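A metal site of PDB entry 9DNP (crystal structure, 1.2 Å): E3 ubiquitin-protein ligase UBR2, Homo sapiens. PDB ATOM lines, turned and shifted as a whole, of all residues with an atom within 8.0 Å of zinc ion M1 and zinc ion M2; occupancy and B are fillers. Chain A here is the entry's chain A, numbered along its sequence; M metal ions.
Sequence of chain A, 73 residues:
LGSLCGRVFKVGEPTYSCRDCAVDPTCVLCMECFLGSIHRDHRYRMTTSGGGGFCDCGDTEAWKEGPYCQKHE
Zinc ion M2 is bound by a ring nitrogen (ND1) of His 72, at 2.1 Å.
The side-chain sulfur (SG) of Cys 57 binds zinc ion M2.
SG of Cys 69 binds zinc ion M2, at 2.3 Å.
Zinc ion M2 is bound by SG of Cys 33, at 2.4 Å.
Zinc ion M2 has four donor atoms within binding distance.
SG of Cys 55 binds zinc ion M1 (2.3 Å).
SG of Cys 5 binds zinc ion M1 (2.3 Å).
Zinc ion M1 is bound by SG of Cys 30 (2.3 Å).
Zinc ion M1 is bound by SG of Cys 33, at 2.4 Å.
Zinc ion M1 has four donor atoms within binding distance.
The backbone NH (N) of Cys 57 sits close to the side-chain sulfur (SG) of Cys 55, at 3.4 Å.
SG of Cys 69 sits close to N of Lys 71 (3.4 Å).
N of Cys 55 lies within hydrogen-bond range of O of Arg 7 (2.9 Å).
SG of Cys 5 lies close to N of Arg 7 (3.8 Å).
The backbone carbonyl oxygen of His 72 is in hydrogen-bond range of the backbone NH of Ser 3 (2.8 Å).
SG of Cys 30 sits close to NE of Arg 7 (3.7 Å).
Of the 28 residues printed, 4 come within 4 Å of zinc ion M2.
Along chain A the residues within 4 Å of zinc ion M1 span positions 5 to 55.
The nearest printed residue that does not touch zinc ion M1 is Cys 57 (4.2 Å).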
ATOM      1  N   SER A   3      36.014  19.482 -29.036  1.00  0.00           N
ATOM      2  CA  SER A   3      36.620  20.801 -28.877  1.00  0.00           C
ATOM      3  C   SER A   3      35.617  21.737 -28.216  1.00  0.00           C
ATOM      4  O   SER A   3      34.426  21.439 -28.097  1.00  0.00           O
ATOM      5  CB  SER A   3      37.140  21.366 -30.215  1.00  0.00           C
ATOM      6  OG  SER A   3      36.133  21.364 -31.201  1.00  0.00           O
ATOM      7  N   LEU A   4      36.128  22.875 -27.754  1.00  0.00           N
ATOM      8  CA  LEU A   4      35.369  23.763 -26.874  1.00  0.00           C
ATOM      9  C   LEU A   4      34.683  24.840 -27.687  1.00  0.00           C
ATOM     10  O   LEU A   4      35.337  25.588 -28.424  1.00  0.00           O
ATOM     11  CB  LEU A   4      36.311  24.402 -25.856  1.00  0.00           C
ATOM     12  CG  LEU A   4      35.741  25.261 -24.717  1.00  0.00           C
ATOM     13  CD1 LEU A   4      34.682  24.520 -23.927  1.00  0.00           C
ATOM     14  CD2 LEU A   4      36.849  25.744 -23.791  1.00  0.00           C
ATOM     15  N   CYS A   5      33.352  24.961 -27.542  1.00  0.00           N
ATOM     16  CA  CYS A   5      32.725  26.237 -27.858  1.00  0.00           C
ATOM     17  C   CYS A   5      32.916  27.178 -26.675  1.00  0.00           C
ATOM     18  O   CYS A   5      33.722  28.104 -26.742  1.00  0.00           O
ATOM     19  CB  CYS A   5      31.232  26.120 -28.174  1.00  0.00           C
ATOM     20  SG  CYS A   5      30.478  27.745 -28.579  1.00  0.00           S
ATOM     21  N   GLY A   6      32.121  26.973 -25.610  1.00  0.00           N
ATOM     22  CA  GLY A   6      32.232  27.692 -24.362  1.00  0.00           C
ATOM     23  C   GLY A   6      31.918  29.168 -24.388  1.00  0.00           C
ATOM     24  O   GLY A   6      32.113  29.847 -23.383  1.00  0.00           O
ATOM     25  N   ARG A   7      31.419  29.698 -25.506  1.00  0.00           N
ATOM     26  CA  ARG A   7      31.425  31.145 -25.675  1.00  0.00           C
ATOM     27  C   ARG A   7      30.341  31.834 -24.854  1.00  0.00           C
ATOM     28  O   ARG A   7      29.260  31.283 -24.609  1.00  0.00           O
ATOM     29  CB  ARG A   7      31.314  31.482 -27.157  1.00  0.00           C
ATOM     30  CG  ARG A   7      29.933  31.377 -27.723  1.00  0.00           C
ATOM     31  CD  ARG A   7      29.976  32.019 -29.101  1.00  0.00           C
ATOM     32  NE  ARG A   7      28.694  32.041 -29.787  1.00  0.00           N
ATOM     33  CZ  ARG A   7      27.749  32.953 -29.543  1.00  0.00           C
ATOM     34  NH1 ARG A   7      27.887  33.839 -28.558  1.00  0.00           N
ATOM     35  NH2 ARG A   7      26.672  32.989 -30.306  1.00  0.00           N
ATOM     36  N   VAL A   8      30.653  33.054 -24.411  1.00  0.00           N
ATOM     37  CA  VAL A   8      29.720  33.875 -23.654  1.00  0.00           C
ATOM     38  C   VAL A   8      28.723  34.500 -24.613  1.00  0.00           C
ATOM     39  O   VAL A   8      29.014  34.714 -25.796  1.00  0.00           O
ATOM     40  CB  VAL A   8      30.526  34.943 -22.866  1.00  0.00           C
ATOM     41  CG1 VAL A   8      29.633  35.962 -22.163  1.00  0.00           C
ATOM     42  CG2 VAL A   8      31.477  34.273 -21.893  1.00  0.00           C
ATOM     43  N   PHE A   9      27.501  34.726 -24.137  1.00  0.00           N
ATOM     44  CA  PHE A   9      26.485  35.406 -24.929  1.00  0.00           C
ATOM     45  C   PHE A   9      26.555  36.908 -24.723  1.00  0.00           C
ATOM     46  O   PHE A   9      26.750  37.390 -23.601  1.00  0.00           O
ATOM     47  CB  PHE A   9      25.096  34.897 -24.554  1.00  0.00           C
ATOM     48  CG  PHE A   9      24.833  33.489 -25.009  1.00  0.00           C
ATOM     49  CD1 PHE A   9      24.689  33.228 -26.361  1.00  0.00           C
ATOM     50  CD2 PHE A   9      24.780  32.445 -24.106  1.00  0.00           C
ATOM     51  CE1 PHE A   9      24.471  31.933 -26.814  1.00  0.00           C
ATOM     52  CE2 PHE A   9      24.569  31.130 -24.552  1.00  0.00           C
ATOM     53  CZ  PHE A   9      24.427  30.885 -25.914  1.00  0.00           C
ATOM     54  N   VAL A  28      21.626  25.580 -22.784  1.00  0.00           N
ATOM     55  CA  VAL A  28      21.437  26.314 -24.032  1.00  0.00           C
ATOM     56  C   VAL A  28      22.616  26.096 -24.969  1.00  0.00           C
ATOM     57  O   VAL A  28      23.750  25.831 -24.554  1.00  0.00           O
ATOM     58  CB  VAL A  28      21.234  27.834 -23.827  1.00  0.00           C
ATOM     59  CG1 VAL A  28      19.887  28.098 -23.197  1.00  0.00           C
ATOM     60  CG2 VAL A  28      22.347  28.404 -22.990  1.00  0.00           C
ATOM     61  N   LEU A  29      22.328  26.220 -26.273  1.00  0.00           N
ATOM     62  CA  LEU A  29      23.334  26.258 -27.323  1.00  0.00           C
ATOM     63  C   LEU A  29      23.285  27.616 -27.999  1.00  0.00           C
ATOM     64  O   LEU A  29      22.212  28.227 -28.139  1.00  0.00           O
ATOM     65  CB  LEU A  29      23.026  25.196 -28.378  1.00  0.00           C
ATOM     66  CG  LEU A  29      23.097  23.769 -27.850  1.00  0.00           C
ATOM     67  CD1 LEU A  29      22.625  22.809 -28.943  1.00  0.00           C
ATOM     68  CD2 LEU A  29      24.491  23.417 -27.377  1.00  0.00           C
ATOM     69  N   CYS A  30      24.460  28.100 -28.415  1.00  0.00           N
ATOM     70  CA  CYS A  30      24.525  29.277 -29.252  1.00  0.00           C
ATOM     71  C   CYS A  30      23.944  28.943 -30.631  1.00  0.00           C
ATOM     72  O   CYS A  30      23.675  27.781 -30.951  1.00  0.00           O
ATOM     73  CB  CYS A  30      25.963  29.802 -29.379  1.00  0.00           C
ATOM     74  SG  CYS A  30      27.112  28.792 -30.347  1.00  0.00           S
ATOM     75  N   MET A  31      23.753  29.974 -31.445  1.00  0.00           N
ATOM     76  CA  MET A  31      23.102  29.766 -32.727  1.00  0.00           C
ATOM     77  C   MET A  31      23.903  28.819 -33.617  1.00  0.00           C
ATOM     78  O   MET A  31      23.358  27.891 -34.206  1.00  0.00           O
ATOM     79  CB  MET A  31      22.898  31.106 -33.422  1.00  0.00           C
ATOM     80  CG  MET A  31      22.272  30.997 -34.785  1.00  0.00           C
ATOM     81  SD  MET A  31      21.889  32.651 -35.423  1.00  0.00           S
ATOM     82  CE  MET A  31      21.289  32.242 -37.064  1.00  0.00           C
ATOM     83  N   GLU A  32      25.222  29.013 -33.673  1.00  0.00           N
ATOM     84  CA  GLU A  32      26.049  28.170 -34.544  1.00  0.00           C
ATOM     85  C   GLU A  32      25.984  26.705 -34.104  1.00  0.00           C
ATOM     86  O   GLU A  32      25.871  25.793 -34.934  1.00  0.00           O
ATOM     87  CB  GLU A  32      27.492  28.684 -34.550  1.00  0.00           C
ATOM     88  CG  GLU A  32      28.479  27.733 -35.181  1.00  0.00           C
ATOM     89  CD  GLU A  32      29.933  28.141 -34.993  1.00  0.00           C
ATOM     90  OE1 GLU A  32      30.273  28.946 -34.085  1.00  0.00           O
ATOM     91  OE2 GLU A  32      30.750  27.590 -35.751  1.00  0.00           O
ATOM     92  N   CYS A  33      26.070  26.469 -32.790  1.00  0.00           N
ATOM     93  CA  CYS A  33      26.053  25.100 -32.301  1.00  0.00           C
ATOM     94  C   CYS A  33      24.673  24.479 -32.477  1.00  0.00           C
ATOM     95  O   CYS A  33      24.547  23.310 -32.860  1.00  0.00           O
ATOM     96  CB  CYS A  33      26.497  25.077 -30.839  1.00  0.00           C
ATOM     97  SG  CYS A  33      28.271  25.486 -30.667  1.00  0.00           S
ATOM     98  N   PHE A  34      23.627  25.261 -32.215  1.00  0.00           N
ATOM     99  CA  PHE A  34      22.279  24.720 -32.388  1.00  0.00           C
ATOM    100  C   PHE A  34      22.043  24.289 -33.825  1.00  0.00           C
ATOM    101  O   PHE A  34      21.569  23.180 -34.077  1.00  0.00           O
ATOM    102  CB  PHE A  34      21.242  25.761 -31.969  1.00  0.00           C
ATOM    103  CG  PHE A  34      19.831  25.295 -32.167  1.00  0.00           C
ATOM    104  CD1 PHE A  34      19.309  24.321 -31.331  1.00  0.00           C
ATOM    105  CD2 PHE A  34      19.052  25.818 -33.175  1.00  0.00           C
ATOM    106  CE1 PHE A  34      18.013  23.882 -31.502  1.00  0.00           C
ATOM    107  CE2 PHE A  34      17.748  25.382 -33.342  1.00  0.00           C
ATOM    108  CZ  PHE A  34      17.239  24.409 -32.503  1.00  0.00           C
ATOM    109  N   GLY A  36      24.038  23.434 -36.088  1.00  0.00           N
ATOM    110  CA  GLY A  36      24.878  22.327 -36.500  1.00  0.00           C
ATOM    111  C   GLY A  36      24.730  21.090 -35.641  1.00  0.00           C
ATOM    112  O   GLY A  36      25.580  20.198 -35.676  1.00  0.00           O
ATOM    113  N   SER A  37      23.652  21.028 -34.858  1.00  0.00           N
ATOM    114  CA  SER A  37      23.389  19.916 -33.951  1.00  0.00           C
ATOM    115  C   SER A  37      22.152  19.150 -34.379  1.00  0.00           C
ATOM    116  O   SER A  37      21.366  19.602 -35.215  1.00  0.00           O
ATOM    117  CB  SER A  37      23.197  20.417 -32.518  1.00  0.00           C
ATOM    118  OG  SER A  37      21.922  21.015 -32.348  1.00  0.00           O
ATOM    119  N   PHE A  54      26.678  31.236 -21.073  1.00  0.00           N
ATOM    120  CA  PHE A  54      27.601  30.640 -22.021  1.00  0.00           C
ATOM    121  C   PHE A  54      26.947  29.447 -22.699  1.00  0.00           C
ATOM    122  O   PHE A  54      26.026  28.818 -22.164  1.00  0.00           O
ATOM    123  CB  PHE A  54      28.926  30.229 -21.367  1.00  0.00           C
ATOM    124  CG  PHE A  54      28.764  29.342 -20.146  1.00  0.00           C
ATOM    125  CD1 PHE A  54      28.571  29.884 -18.879  1.00  0.00           C
ATOM    126  CD2 PHE A  54      28.755  27.972 -20.278  1.00  0.00           C
ATOM    127  CE1 PHE A  54      28.426  29.040 -17.759  1.00  0.00           C
ATOM    128  CE2 PHE A  54      28.603  27.139 -19.159  1.00  0.00           C
ATOM    129  CZ  PHE A  54      28.438  27.688 -17.914  1.00  0.00           C
ATOM    130  N   CYS A  55      27.450  29.122 -23.880  1.00  0.00           N
ATOM    131  CA  CYS A  55      26.989  27.961 -24.623  1.00  0.00           C
ATOM    132  C   CYS A  55      27.414  26.669 -23.943  1.00  0.00           C
ATOM    133  O   CYS A  55      28.563  26.527 -23.498  1.00  0.00           O
ATOM    134  CB  CYS A  55      27.601  28.005 -26.007  1.00  0.00           C
ATOM    135  SG  CYS A  55      27.137  26.653 -27.106  1.00  0.00           S
ATOM    136  N   ASP A  56      26.499  25.701 -23.927  1.00  0.00           N
ATOM    137  CA  ASP A  56      26.731  24.406 -23.287  1.00  0.00           C
ATOM    138  C   ASP A  56      27.092  23.287 -24.255  1.00  0.00           C
ATOM    139  O   ASP A  56      27.019  22.105 -23.894  1.00  0.00           O
ATOM    140  CB  ASP A  56      25.510  24.004 -22.452  1.00  0.00           C
ATOM    141  CG  ASP A  56      25.217  24.973 -21.332  1.00  0.00           C
ATOM    142  OD1 ASP A  56      26.133  25.244 -20.521  1.00  0.00           O
ATOM    143  OD2 ASP A  56      24.067  25.449 -21.245  1.00  0.00           O
ATOM    144  N   CYS A  57      27.448  23.630 -25.484  1.00  0.00           N
ATOM    145  CA  CYS A  57      27.847  22.603 -26.447  1.00  0.00           C
ATOM    146  C   CYS A  57      29.014  21.801 -25.886  1.00  0.00           C
ATOM    147  O   CYS A  57      29.990  22.379 -25.409  1.00  0.00           O
ATOM    148  CB  CYS A  57      28.284  23.263 -27.740  1.00  0.00           C
ATOM    149  SG  CYS A  57      28.763  22.052 -29.012  1.00  0.00           S
ATOM    150  N   GLY A  58      28.886  20.483 -25.915  1.00  0.00           N
ATOM    151  CA  GLY A  58      29.951  19.630 -25.457  1.00  0.00           C
ATOM    152  C   GLY A  58      29.977  19.373 -23.975  1.00  0.00           C
ATOM    153  O   GLY A  58      30.893  18.706 -23.491  1.00  0.00           O
ATOM    154  N   PRO A  67      25.206  15.865 -27.208  1.00  0.00           N
ATOM    155  CA  PRO A  67      25.831  17.007 -26.523  1.00  0.00           C
ATOM    156  C   PRO A  67      26.705  17.872 -27.414  1.00  0.00           C
ATOM    157  O   PRO A  67      26.921  19.042 -27.090  1.00  0.00           O
ATOM    158  CB  PRO A  67      26.651  16.363 -25.398  1.00  0.00           C
ATOM    159  CG  PRO A  67      26.931  14.977 -25.909  1.00  0.00           C
ATOM    160  CD  PRO A  67      25.699  14.585 -26.670  1.00  0.00           C
ATOM    161  N   TYR A  68      27.215  17.340 -28.529  1.00  0.00           N
ATOM    162  CA  TYR A  68      28.152  18.044 -29.403  1.00  0.00           C
ATOM    163  C   TYR A  68      27.497  18.342 -30.741  1.00  0.00           C
ATOM    164  O   TYR A  68      26.803  17.488 -31.310  1.00  0.00           O
ATOM    165  CB  TYR A  68      29.356  17.157 -29.713  1.00  0.00           C
ATOM    166  CG  TYR A  68      30.174  16.763 -28.524  1.00  0.00           C
ATOM    167  CD1 TYR A  68      31.151  17.615 -28.021  1.00  0.00           C
ATOM    168  CD2 TYR A  68      29.964  15.549 -27.872  1.00  0.00           C
ATOM    169  CE1 TYR A  68      31.918  17.254 -26.921  1.00  0.00           C
ATOM    170  CE2 TYR A  68      30.709  15.191 -26.772  1.00  0.00           C
ATOM    171  CZ  TYR A  68      31.682  16.044 -26.306  1.00  0.00           C
ATOM    172  OH  TYR A  68      32.427  15.687 -25.206  1.00  0.00           O
ATOM    173  N   CYS A  69      27.738  19.551 -31.240  1.00  0.00           N
ATOM    174  CA  CYS A  69      27.368  19.894 -32.606  1.00  0.00           C
ATOM    175  C   CYS A  69      28.433  19.362 -33.577  1.00  0.00           C
ATOM    176  O   CYS A  69      29.477  18.835 -33.186  1.00  0.00           O
ATOM    177  CB  CYS A  69      27.201  21.401 -32.746  1.00  0.00           C
ATOM    178  SG  CYS A  69      28.786  22.289 -32.808  1.00  0.00           S
ATOM    179  N   GLN A  70      28.164  19.532 -34.878  1.00  0.00           N
ATOM    180  CA  GLN A  70      29.054  19.009 -35.908  1.00  0.00           C
ATOM    181  C   GLN A  70      30.463  19.606 -35.804  1.00  0.00           C
ATOM    182  O   GLN A  70      31.438  18.919 -36.096  1.00  0.00           O
ATOM    183  CB  GLN A  70      28.458  19.272 -37.292  1.00  0.00           C
ATOM    184  CG  GLN A  70      27.953  20.704 -37.523  1.00  0.00           C
ATOM    185  CD  GLN A  70      27.035  20.860 -38.756  1.00  0.00           C
ATOM    186  OE1 GLN A  70      27.142  21.819 -39.519  1.00  0.00           O
ATOM    187  NE2 GLN A  70      26.112  19.909 -38.927  1.00  0.00           N
ATOM    188  N   LYS A  71      30.572  20.861 -35.377  1.00  0.00           N
ATOM    189  CA  LYS A  71      31.892  21.480 -35.331  1.00  0.00           C
ATOM    190  C   LYS A  71      32.718  20.997 -34.152  1.00  0.00           C
ATOM    191  O   LYS A  71      33.944  20.863 -34.261  1.00  0.00           O
ATOM    192  CB  LYS A  71      31.751  23.000 -35.272  1.00  0.00           C
ATOM    193  CG  LYS A  71      33.057  23.725 -35.247  1.00  0.00           C
ATOM    194  CD  LYS A  71      32.835  25.211 -35.103  1.00  0.00           C
ATOM    195  CE  LYS A  71      34.104  25.987 -35.330  1.00  0.00           C
ATOM    196  NZ  LYS A  71      33.768  27.426 -35.479  1.00  0.00           N
ATOM    197  N   HIS A  72      32.079  20.741 -33.005  1.00  0.00           N
ATOM    198  CA  HIS A  72      32.817  20.545 -31.776  1.00  0.00           C
ATOM    199  C   HIS A  72      32.946  19.083 -31.373  1.00  0.00           C
ATOM    200  O   HIS A  72      33.697  18.787 -30.441  1.00  0.00           O
ATOM    201  CB  HIS A  72      32.196  21.393 -30.664  1.00  0.00           C
ATOM    202  CG  HIS A  72      32.351  22.854 -30.899  1.00  0.00           C
ATOM    203  ND1 HIS A  72      31.268  23.691 -31.075  1.00  0.00           N
ATOM    204  CD2 HIS A  72      33.449  23.619 -31.060  1.00  0.00           C
ATOM    205  CE1 HIS A  72      31.699  24.924 -31.306  1.00  0.00           C
ATOM    206  NE2 HIS A  72      33.025  24.898 -31.315  1.00  0.00           N
ATOM    207  N   GLU A  73      32.260  18.187 -32.070  1.00  0.00           N
ATOM    208  CA  GLU A  73      32.379  16.764 -31.799  1.00  0.00           C
ATOM    209  C   GLU A  73      33.815  16.275 -32.067  1.00  0.00           C
ATOM    210  O   GLU A  73      34.213  15.224 -31.576  1.00  0.00           O
ATOM    211  CB  GLU A  73      31.354  15.982 -32.621  1.00  0.00           C
ATOM    212  CG  GLU A  73      31.627  15.949 -34.120  1.00  0.00           C
ATOM    213  CD  GLU A  73      30.543  15.202 -34.896  1.00  0.00           C
ATOM    214  OE1 GLU A  73      30.638  15.132 -36.140  1.00  0.00           O
ATOM    215  OE2 GLU A  73      29.609  14.686 -34.255  1.00  0.00           O
ATOM    216  OXT GLU A  73      34.607  16.932 -32.755  1.00  0.00           O
HETATM  217 ZN    ZN M   1      28.265  27.251 -29.032  1.00  0.00          ZN
HETATM  218 ZN    ZN M   2      29.240  23.350 -30.814  1.00  0.00          ZN
